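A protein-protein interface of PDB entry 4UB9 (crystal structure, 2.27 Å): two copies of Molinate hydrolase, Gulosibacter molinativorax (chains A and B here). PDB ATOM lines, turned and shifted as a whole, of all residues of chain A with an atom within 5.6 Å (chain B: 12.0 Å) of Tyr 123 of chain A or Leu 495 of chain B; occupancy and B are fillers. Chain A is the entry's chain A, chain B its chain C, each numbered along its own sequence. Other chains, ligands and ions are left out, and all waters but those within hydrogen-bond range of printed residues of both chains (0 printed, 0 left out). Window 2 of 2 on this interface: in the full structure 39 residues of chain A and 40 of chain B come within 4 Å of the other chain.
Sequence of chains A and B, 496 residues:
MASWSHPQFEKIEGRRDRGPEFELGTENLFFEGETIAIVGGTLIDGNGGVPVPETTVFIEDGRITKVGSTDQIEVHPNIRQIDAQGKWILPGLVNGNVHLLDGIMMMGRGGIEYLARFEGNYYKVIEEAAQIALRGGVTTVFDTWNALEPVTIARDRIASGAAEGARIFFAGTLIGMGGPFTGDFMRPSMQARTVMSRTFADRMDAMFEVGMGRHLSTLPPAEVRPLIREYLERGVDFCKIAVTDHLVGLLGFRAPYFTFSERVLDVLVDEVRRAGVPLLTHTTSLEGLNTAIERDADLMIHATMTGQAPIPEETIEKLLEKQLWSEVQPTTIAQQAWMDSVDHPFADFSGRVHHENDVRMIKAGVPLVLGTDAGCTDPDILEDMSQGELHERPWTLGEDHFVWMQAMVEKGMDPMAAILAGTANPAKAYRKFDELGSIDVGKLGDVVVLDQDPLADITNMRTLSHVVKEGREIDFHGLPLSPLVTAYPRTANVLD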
ATOM      1  N   GLY A 120     -33.163   2.866  27.027  1.00  0.00           N
ATOM      2  CA  GLY A 120     -32.442   1.702  27.529  1.00  0.00           C
ATOM      3  C   GLY A 120     -31.146   1.456  26.753  1.00  0.00           C
ATOM      4  O   GLY A 120     -30.253   0.781  27.256  1.00  0.00           O
ATOM      5  N   ASN A 121     -31.068   1.978  25.530  1.00  0.00           N
ATOM      6  CA  ASN A 121     -29.946   1.721  24.643  1.00  0.00           C
ATOM      7  C   ASN A 121     -29.319   2.928  23.997  1.00  0.00           C
ATOM      8  O   ASN A 121     -28.702   2.833  22.930  1.00  0.00           O
ATOM      9  CB  ASN A 121     -30.392   0.799  23.507  1.00  0.00           C
ATOM     10  CG  ASN A 121     -30.594  -0.620  23.947  1.00  0.00           C
ATOM     11  OD1 ASN A 121     -31.699  -1.142  23.840  1.00  0.00           O
ATOM     12  ND2 ASN A 121     -29.580  -1.212  24.534  1.00  0.00           N
ATOM     13  N   TYR A 122     -29.498   4.086  24.600  1.00  0.00           N
ATOM     14  CA  TYR A 122     -29.061   5.306  23.936  1.00  0.00           C
ATOM     15  C   TYR A 122     -27.565   5.252  23.636  1.00  0.00           C
ATOM     16  O   TYR A 122     -27.149   5.661  22.552  1.00  0.00           O
ATOM     17  CB  TYR A 122     -29.426   6.542  24.755  1.00  0.00           C
ATOM     18  CG  TYR A 122     -30.909   6.749  24.920  1.00  0.00           C
ATOM     19  CD1 TYR A 122     -31.766   6.760  23.825  1.00  0.00           C
ATOM     20  CD2 TYR A 122     -31.449   6.970  26.166  1.00  0.00           C
ATOM     21  CE1 TYR A 122     -33.126   6.967  23.977  1.00  0.00           C
ATOM     22  CE2 TYR A 122     -32.790   7.193  26.338  1.00  0.00           C
ATOM     23  CZ  TYR A 122     -33.639   7.189  25.255  1.00  0.00           C
ATOM     24  OH  TYR A 122     -34.983   7.395  25.455  1.00  0.00           O
ATOM     25  N   TYR A 123     -26.770   4.680  24.546  1.00  0.00           N
ATOM     26  CA  TYR A 123     -25.326   4.612  24.312  1.00  0.00           C
ATOM     27  C   TYR A 123     -25.015   3.781  23.067  1.00  0.00           C
ATOM     28  O   TYR A 123     -24.057   4.077  22.346  1.00  0.00           O
ATOM     29  CB  TYR A 123     -24.529   4.094  25.514  1.00  0.00           C
ATOM     30  CG  TYR A 123     -24.664   2.618  25.862  1.00  0.00           C
ATOM     31  CD1 TYR A 123     -25.751   2.166  26.589  1.00  0.00           C
ATOM     32  CD2 TYR A 123     -23.726   1.695  25.450  1.00  0.00           C
ATOM     33  CE1 TYR A 123     -25.912   0.821  26.879  1.00  0.00           C
ATOM     34  CE2 TYR A 123     -23.843   0.351  25.778  1.00  0.00           C
ATOM     35  CZ  TYR A 123     -24.943  -0.081  26.498  1.00  0.00           C
ATOM     36  OH  TYR A 123     -25.084  -1.404  26.867  1.00  0.00           O
ATOM     37  N   LYS A 124     -25.823   2.762  22.802  1.00  0.00           N
ATOM     38  CA  LYS A 124     -25.623   1.926  21.591  1.00  0.00           C
ATOM     39  C   LYS A 124     -26.042   2.639  20.338  1.00  0.00           C
ATOM     40  O   LYS A 124     -25.459   2.444  19.284  1.00  0.00           O
ATOM     41  CB  LYS A 124     -26.385   0.629  21.698  1.00  0.00           C
ATOM     42  CG  LYS A 124     -25.742  -0.332  22.664  1.00  0.00           C
ATOM     43  CD  LYS A 124     -26.487  -1.649  22.763  1.00  0.00           C
ATOM     44  CE  LYS A 124     -25.723  -2.570  23.688  1.00  0.00           C
ATOM     45  NZ  LYS A 124     -26.613  -3.575  24.311  1.00  0.00           N
ATOM     46  N   VAL A 125     -27.075   3.469  20.454  1.00  0.00           N
ATOM     47  CA  VAL A 125     -27.487   4.297  19.331  1.00  0.00           C
ATOM     48  C   VAL A 125     -26.310   5.205  18.945  1.00  0.00           C
ATOM     49  O   VAL A 125     -26.007   5.429  17.767  1.00  0.00           O
ATOM     50  CB  VAL A 125     -28.690   5.175  19.681  1.00  0.00           C
ATOM     51  CG1 VAL A 125     -28.977   6.209  18.590  1.00  0.00           C
ATOM     52  CG2 VAL A 125     -29.894   4.307  19.922  1.00  0.00           C
ATOM     53  N   ILE A 126     -25.669   5.759  19.963  1.00  0.00           N
ATOM     54  CA  ILE A 126     -24.583   6.692  19.752  1.00  0.00           C
ATOM     55  C   ILE A 126     -23.394   5.957  19.114  1.00  0.00           C
ATOM     56  O   ILE A 126     -22.765   6.446  18.186  1.00  0.00           O
ATOM     57  CB  ILE A 126     -24.185   7.372  21.066  1.00  0.00           C
ATOM     58  CG1 ILE A 126     -25.261   8.380  21.451  1.00  0.00           C
ATOM     59  CG2 ILE A 126     -22.844   8.099  20.923  1.00  0.00           C
ATOM     60  CD1 ILE A 126     -25.095   8.967  22.834  1.00  0.00           C
ATOM     61  N   GLU A 127     -23.092   4.767  19.619  1.00  0.00           N
ATOM     62  CA  GLU A 127     -22.003   3.935  19.026  1.00  0.00           C
ATOM     63  C   GLU A 127     -22.295   3.589  17.577  1.00  0.00           C
ATOM     64  O   GLU A 127     -21.447   3.780  16.708  1.00  0.00           O
ATOM     65  CB  GLU A 127     -21.743   2.682  19.833  1.00  0.00           C
ATOM     66  CG  GLU A 127     -21.103   3.026  21.172  1.00  0.00           C
ATOM     67  CD  GLU A 127     -21.148   1.898  22.198  1.00  0.00           C
ATOM     68  OE1 GLU A 127     -21.597   0.780  21.846  1.00  0.00           O
ATOM     69  OE2 GLU A 127     -20.727   2.140  23.360  1.00  0.00           O
ATOM     70  N   GLU A 128     -23.502   3.141  17.314  1.00  0.00           N
ATOM     71  CA  GLU A 128     -23.944   2.870  15.918  1.00  0.00           C
ATOM     72  C   GLU A 128     -23.704   4.102  15.013  1.00  0.00           C
ATOM     73  O   GLU A 128     -23.186   3.989  13.900  1.00  0.00           O
ATOM     74  CB  GLU A 128     -25.425   2.491  15.861  1.00  0.00           C
ATOM     75  CG  GLU A 128     -25.988   2.258  14.462  1.00  0.00           C
ATOM     76  CD  GLU A 128     -27.495   2.014  14.420  1.00  0.00           C
ATOM     77  OE1 GLU A 128     -28.204   2.562  15.290  1.00  0.00           O
ATOM     78  OE2 GLU A 128     -27.997   1.285  13.526  1.00  0.00           O
ATOM     79  N   PRO A 150     -25.358   9.156  28.143  1.00  0.00           N
ATOM     80  CA  PRO A 150     -25.037   8.115  27.160  1.00  0.00           C
ATOM     81  C   PRO A 150     -23.883   8.471  26.251  1.00  0.00           C
ATOM     82  O   PRO A 150     -23.180   7.584  25.818  1.00  0.00           O
ATOM     83  CB  PRO A 150     -26.313   7.988  26.338  1.00  0.00           C
ATOM     84  CG  PRO A 150     -27.091   9.220  26.600  1.00  0.00           C
ATOM     85  CD  PRO A 150     -26.721   9.678  27.968  1.00  0.00           C
ATOM     86  N   ILE A 153     -20.770   7.490  28.307  1.00  0.00           N
ATOM     87  CA  ILE A 153     -20.646   6.020  28.228  1.00  0.00           C
ATOM     88  C   ILE A 153     -20.025   5.564  26.894  1.00  0.00           C
ATOM     89  O   ILE A 153     -19.130   4.726  26.854  1.00  0.00           O
ATOM     90  CB  ILE A 153     -21.994   5.328  28.402  1.00  0.00           C
ATOM     91  CG1 ILE A 153     -22.434   5.485  29.859  1.00  0.00           C
ATOM     92  CG2 ILE A 153     -21.898   3.847  28.053  1.00  0.00           C
ATOM     93  CD1 ILE A 153     -23.864   5.082  30.156  1.00  0.00           C
ATOM     94  N   ALA A 154     -20.542   6.130  25.814  1.00  0.00           N
ATOM     95  CA  ALA A 154     -20.181   5.711  24.456  1.00  0.00           C
ATOM     96  C   ALA A 154     -18.766   6.141  24.101  1.00  0.00           C
ATOM     97  O   ALA A 154     -18.012   5.368  23.520  1.00  0.00           O
ATOM     98  CB  ALA A 154     -21.148   6.268  23.434  1.00  0.00           C
ATOM     99  N   ARG A 157     -16.228   3.950  25.998  1.00  0.00           N
ATOM    100  CA  ARG A 157     -16.136   2.613  25.466  1.00  0.00           C
ATOM    101  C   ARG A 157     -15.399   2.562  24.153  1.00  0.00           C
ATOM    102  O   ARG A 157     -14.652   1.634  23.882  1.00  0.00           O
ATOM    103  CB  ARG A 157     -17.518   1.999  25.347  1.00  0.00           C
ATOM    104  CG  ARG A 157     -17.996   1.469  26.693  1.00  0.00           C
ATOM    105  CD  ARG A 157     -19.493   1.184  26.732  1.00  0.00           C
ATOM    106  NE  ARG A 157     -19.997   0.677  25.454  1.00  0.00           N
ATOM    107  CZ  ARG A 157     -20.040  -0.611  25.098  1.00  0.00           C
ATOM    108  NH1 ARG A 157     -19.588  -1.550  25.901  1.00  0.00           N
ATOM    109  NH2 ARG A 157     -20.510  -0.953  23.907  1.00  0.00           N
ATOM    110  N   PRO B 489     -39.068   1.435  37.240  1.00  0.00           N
ATOM    111  CA  PRO B 489     -38.823   2.539  36.329  1.00  0.00           C
ATOM    112  C   PRO B 489     -38.026   2.116  35.112  1.00  0.00           C
ATOM    113  O   PRO B 489     -37.551   1.011  35.041  1.00  0.00           O
ATOM    114  CB  PRO B 489     -37.954   3.493  37.150  1.00  0.00           C
ATOM    115  CG  PRO B 489     -37.946   2.962  38.531  1.00  0.00           C
ATOM    116  CD  PRO B 489     -38.206   1.500  38.422  1.00  0.00           C
ATOM    117  N   ARG B 490     -37.875   3.040  34.179  1.00  0.00           N
ATOM    118  CA  ARG B 490     -37.228   2.778  32.935  1.00  0.00           C
ATOM    119  C   ARG B 490     -35.866   3.406  32.925  1.00  0.00           C
ATOM    120  O   ARG B 490     -35.707   4.621  32.928  1.00  0.00           O
ATOM    121  CB  ARG B 490     -38.091   3.303  31.802  1.00  0.00           C
ATOM    122  CG  ARG B 490     -39.227   2.346  31.446  1.00  0.00           C
ATOM    123  CD  ARG B 490     -40.345   3.027  30.655  1.00  0.00           C
ATOM    124  NE  ARG B 490     -41.438   2.108  30.361  1.00  0.00           N
ATOM    125  CZ  ARG B 490     -42.626   2.467  29.868  1.00  0.00           C
ATOM    126  NH1 ARG B 490     -42.898   3.738  29.585  1.00  0.00           N
ATOM    127  NH2 ARG B 490     -43.560   1.550  29.682  1.00  0.00           N
ATOM    128  N   THR B 491     -34.849   2.566  32.887  1.00  0.00           N
ATOM    129  CA  THR B 491     -33.478   3.061  32.911  1.00  0.00           C
ATOM    130  C   THR B 491     -33.025   3.396  31.457  1.00  0.00           C
ATOM    131  O   THR B 491     -33.313   2.684  30.493  1.00  0.00           O
ATOM    132  CB  THR B 491     -32.471   2.117  33.638  1.00  0.00           C
ATOM    133  OG1 THR B 491     -31.784   1.315  32.676  1.00  0.00           O
ATOM    134  CG2 THR B 491     -33.124   1.235  34.709  1.00  0.00           C
ATOM    135  N   ALA B 492     -32.312   4.513  31.334  1.00  0.00           N
ATOM    136  CA  ALA B 492     -31.920   5.101  30.039  1.00  0.00           C
ATOM    137  C   ALA B 492     -30.858   4.288  29.275  1.00  0.00           C
ATOM    138  O   ALA B 492     -30.877   4.198  28.032  1.00  0.00           O
ATOM    139  CB  ALA B 492     -31.407   6.510  30.266  1.00  0.00           C
ATOM    140  N   ASN B 493     -29.908   3.750  30.032  1.00  0.00           N
ATOM    141  CA  ASN B 493     -28.776   3.045  29.459  1.00  0.00           C
ATOM    142  C   ASN B 493     -28.493   1.769  30.228  1.00  0.00           C
ATOM    143  O   ASN B 493     -27.759   1.773  31.215  1.00  0.00           O
ATOM    144  CB  ASN B 493     -27.526   3.928  29.427  1.00  0.00           C
ATOM    145  CG  ASN B 493     -27.689   5.123  28.523  1.00  0.00           C
ATOM    146  OD1 ASN B 493     -27.638   4.996  27.293  1.00  0.00           O
ATOM    147  ND2 ASN B 493     -27.963   6.282  29.123  1.00  0.00           N
ATOM    148  N   VAL B 494     -29.079   0.680  29.762  1.00  0.00           N
ATOM    149  CA  VAL B 494     -28.869  -0.630  30.378  1.00  0.00           C
ATOM    150  C   VAL B 494     -27.534  -1.215  29.890  1.00  0.00           C
ATOM    151  O   VAL B 494     -27.352  -1.494  28.700  1.00  0.00           O
ATOM    152  CB  VAL B 494     -30.037  -1.580  30.046  1.00  0.00           C
ATOM    153  CG1 VAL B 494     -29.781  -2.968  30.626  1.00  0.00           C
ATOM    154  CG2 VAL B 494     -31.337  -1.004  30.587  1.00  0.00           C
ATOM    155  N   LEU B 495     -26.615  -1.400  30.821  1.00  0.00           N
ATOM    156  CA  LEU B 495     -25.320  -2.047  30.542  1.00  0.00           C
ATOM    157  C   LEU B 495     -25.455  -3.537  30.826  1.00  0.00           C
ATOM    158  O   LEU B 495     -25.803  -3.920  31.934  1.00  0.00           O
ATOM    159  CB  LEU B 495     -24.251  -1.429  31.430  1.00  0.00           C
ATOM    160  CG  LEU B 495     -24.186   0.091  31.225  1.00  0.00           C
ATOM    161  CD1 LEU B 495     -23.660   0.832  32.455  1.00  0.00           C
ATOM    162  CD2 LEU B 495     -23.376   0.400  29.962  1.00  0.00           C
ATOM    163  N   ASP B 496     -25.189  -4.386  29.837  1.00  0.00           N
ATOM    164  CA  ASP B 496     -25.658  -5.822  29.873  1.00  0.00           C
ATOM    165  C   ASP B 496     -24.578  -6.903  30.090  1.00  0.00           C
ATOM    166  O   ASP B 496     -23.473  -6.607  30.533  1.00  0.00           O
ATOM    167  CB  ASP B 496     -26.468  -6.167  28.610  1.00  0.00           C
ATOM    168  CG  ASP B 496     -25.763  -5.755  27.316  1.00  0.00           C
ATOM    169  OD1 ASP B 496     -24.567  -5.375  27.345  1.00  0.00           O
ATOM    170  OD2 ASP B 496     -26.411  -5.821  26.258  1.00  0.00           O
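Printed residues of chain B that touch a printed residue of chain A: Thr 491, Ala 492, Asn 493, Val 494, Leu 495 and Asp 496.
Hydrophobic or aromatic side chains of chain B within 4 Å of the printed part of chain A: Val 494 and Leu 495.
Of the 13 printed residues of chain A, 7 touch a printed residue of chain B.
Printed residues of chain A that touch a printed residue of chain B: Gly 120, Asn 121, Tyr 122, Tyr 123, Lys 124, Pro 150 and Ile 153.
Printed residues of chain B within 4 Å of Tyr 123 of chain A: Asn 493, Val 494 and Leu 495.
Of chain A, only Tyr 123 (3.7 Å) comes within 4 Å of Leu 495 of chain B.
Of chain B, only Ala 492 comes within 4 Å of Asn 121 of chain A.
No residue of chain B comes within 4 Å of Ile 126 of chain A.
No residue of chain B comes within 4 Å of Glu 127 of chain A.
Printed residues of chain B within 4 Å of Pro 150 of chain A: Asn 493.
Ile 153 of chain A touches just one residue of chain B: Asn 493 (3.9 Å).
No residue of chain B comes within 4 Å of Ala 154 of chain A.
Printed residues of chain A within 4 Å of Thr 491 of chain B: Gly 120 (3.2 Å).
Of the printed residues of chain A, Asp 496 of chain B touches Lys 124.
Arg 490 of chain B touches none of the printed residues of chain A.
The nearest residue of chain B that does not touch Tyr 123 of chain A is Asp 496 of chain B (4.03 Å).
The backbone NH of Gly 120 of chain A lies close to the backbone carbonyl oxygen of Thr 491 of chain B (3.5 Å).
N of Gly 120 of chain A sits at hydrogen-bond distance from O of Ala 492 of chain B (2.8 Å).
The backbone NH (N) of Val 494 of chain B sits at hydrogen-bond distance from the backbone carbonyl oxygen (O) of Gly 120 of chain A.
The backbone NH (N) of Asn 121 of chain A sits at hydrogen-bond distance from the backbone carbonyl oxygen (O) of Ala 492 of chain B (3.4 Å).
The side-chain amide oxygen of Asn 493 of chain B lies within hydrogen-bond range of the backbone NH of Tyr 122 of chain A (3.4 Å).
N of Tyr 123 of chain A is in hydrogen-bond range of OD1 of Asn 493 of chain B (2.9 Å).
The backbone carbonyl oxygen of Val 494 of chain B sits at hydrogen-bond distance from the side-chain hydroxyl of Tyr 123 of chain A, 2.9 Å away.
The side-chain amino group of Lys 124 of chain A is in salt-bridge range of the side-chain carboxylate of Asp 496 of chain B (3.0 Å).
No position is printed for both chains.
Among the printed residues, pairs that only touch across the chains: Tyr 122 of chain A with Ala 492 of chain B (3.4 Å), Pro 150 of chain A with Asn 493 of chain B (3.4 Å), Gly 120 of chain A with Asn 493 of chain B (3.5 Å), Tyr 123 of chain A with Leu 495 of chain B (3.7 Å) and Ile 153 of chain A with Asn 493 of chain B (3.9 Å).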
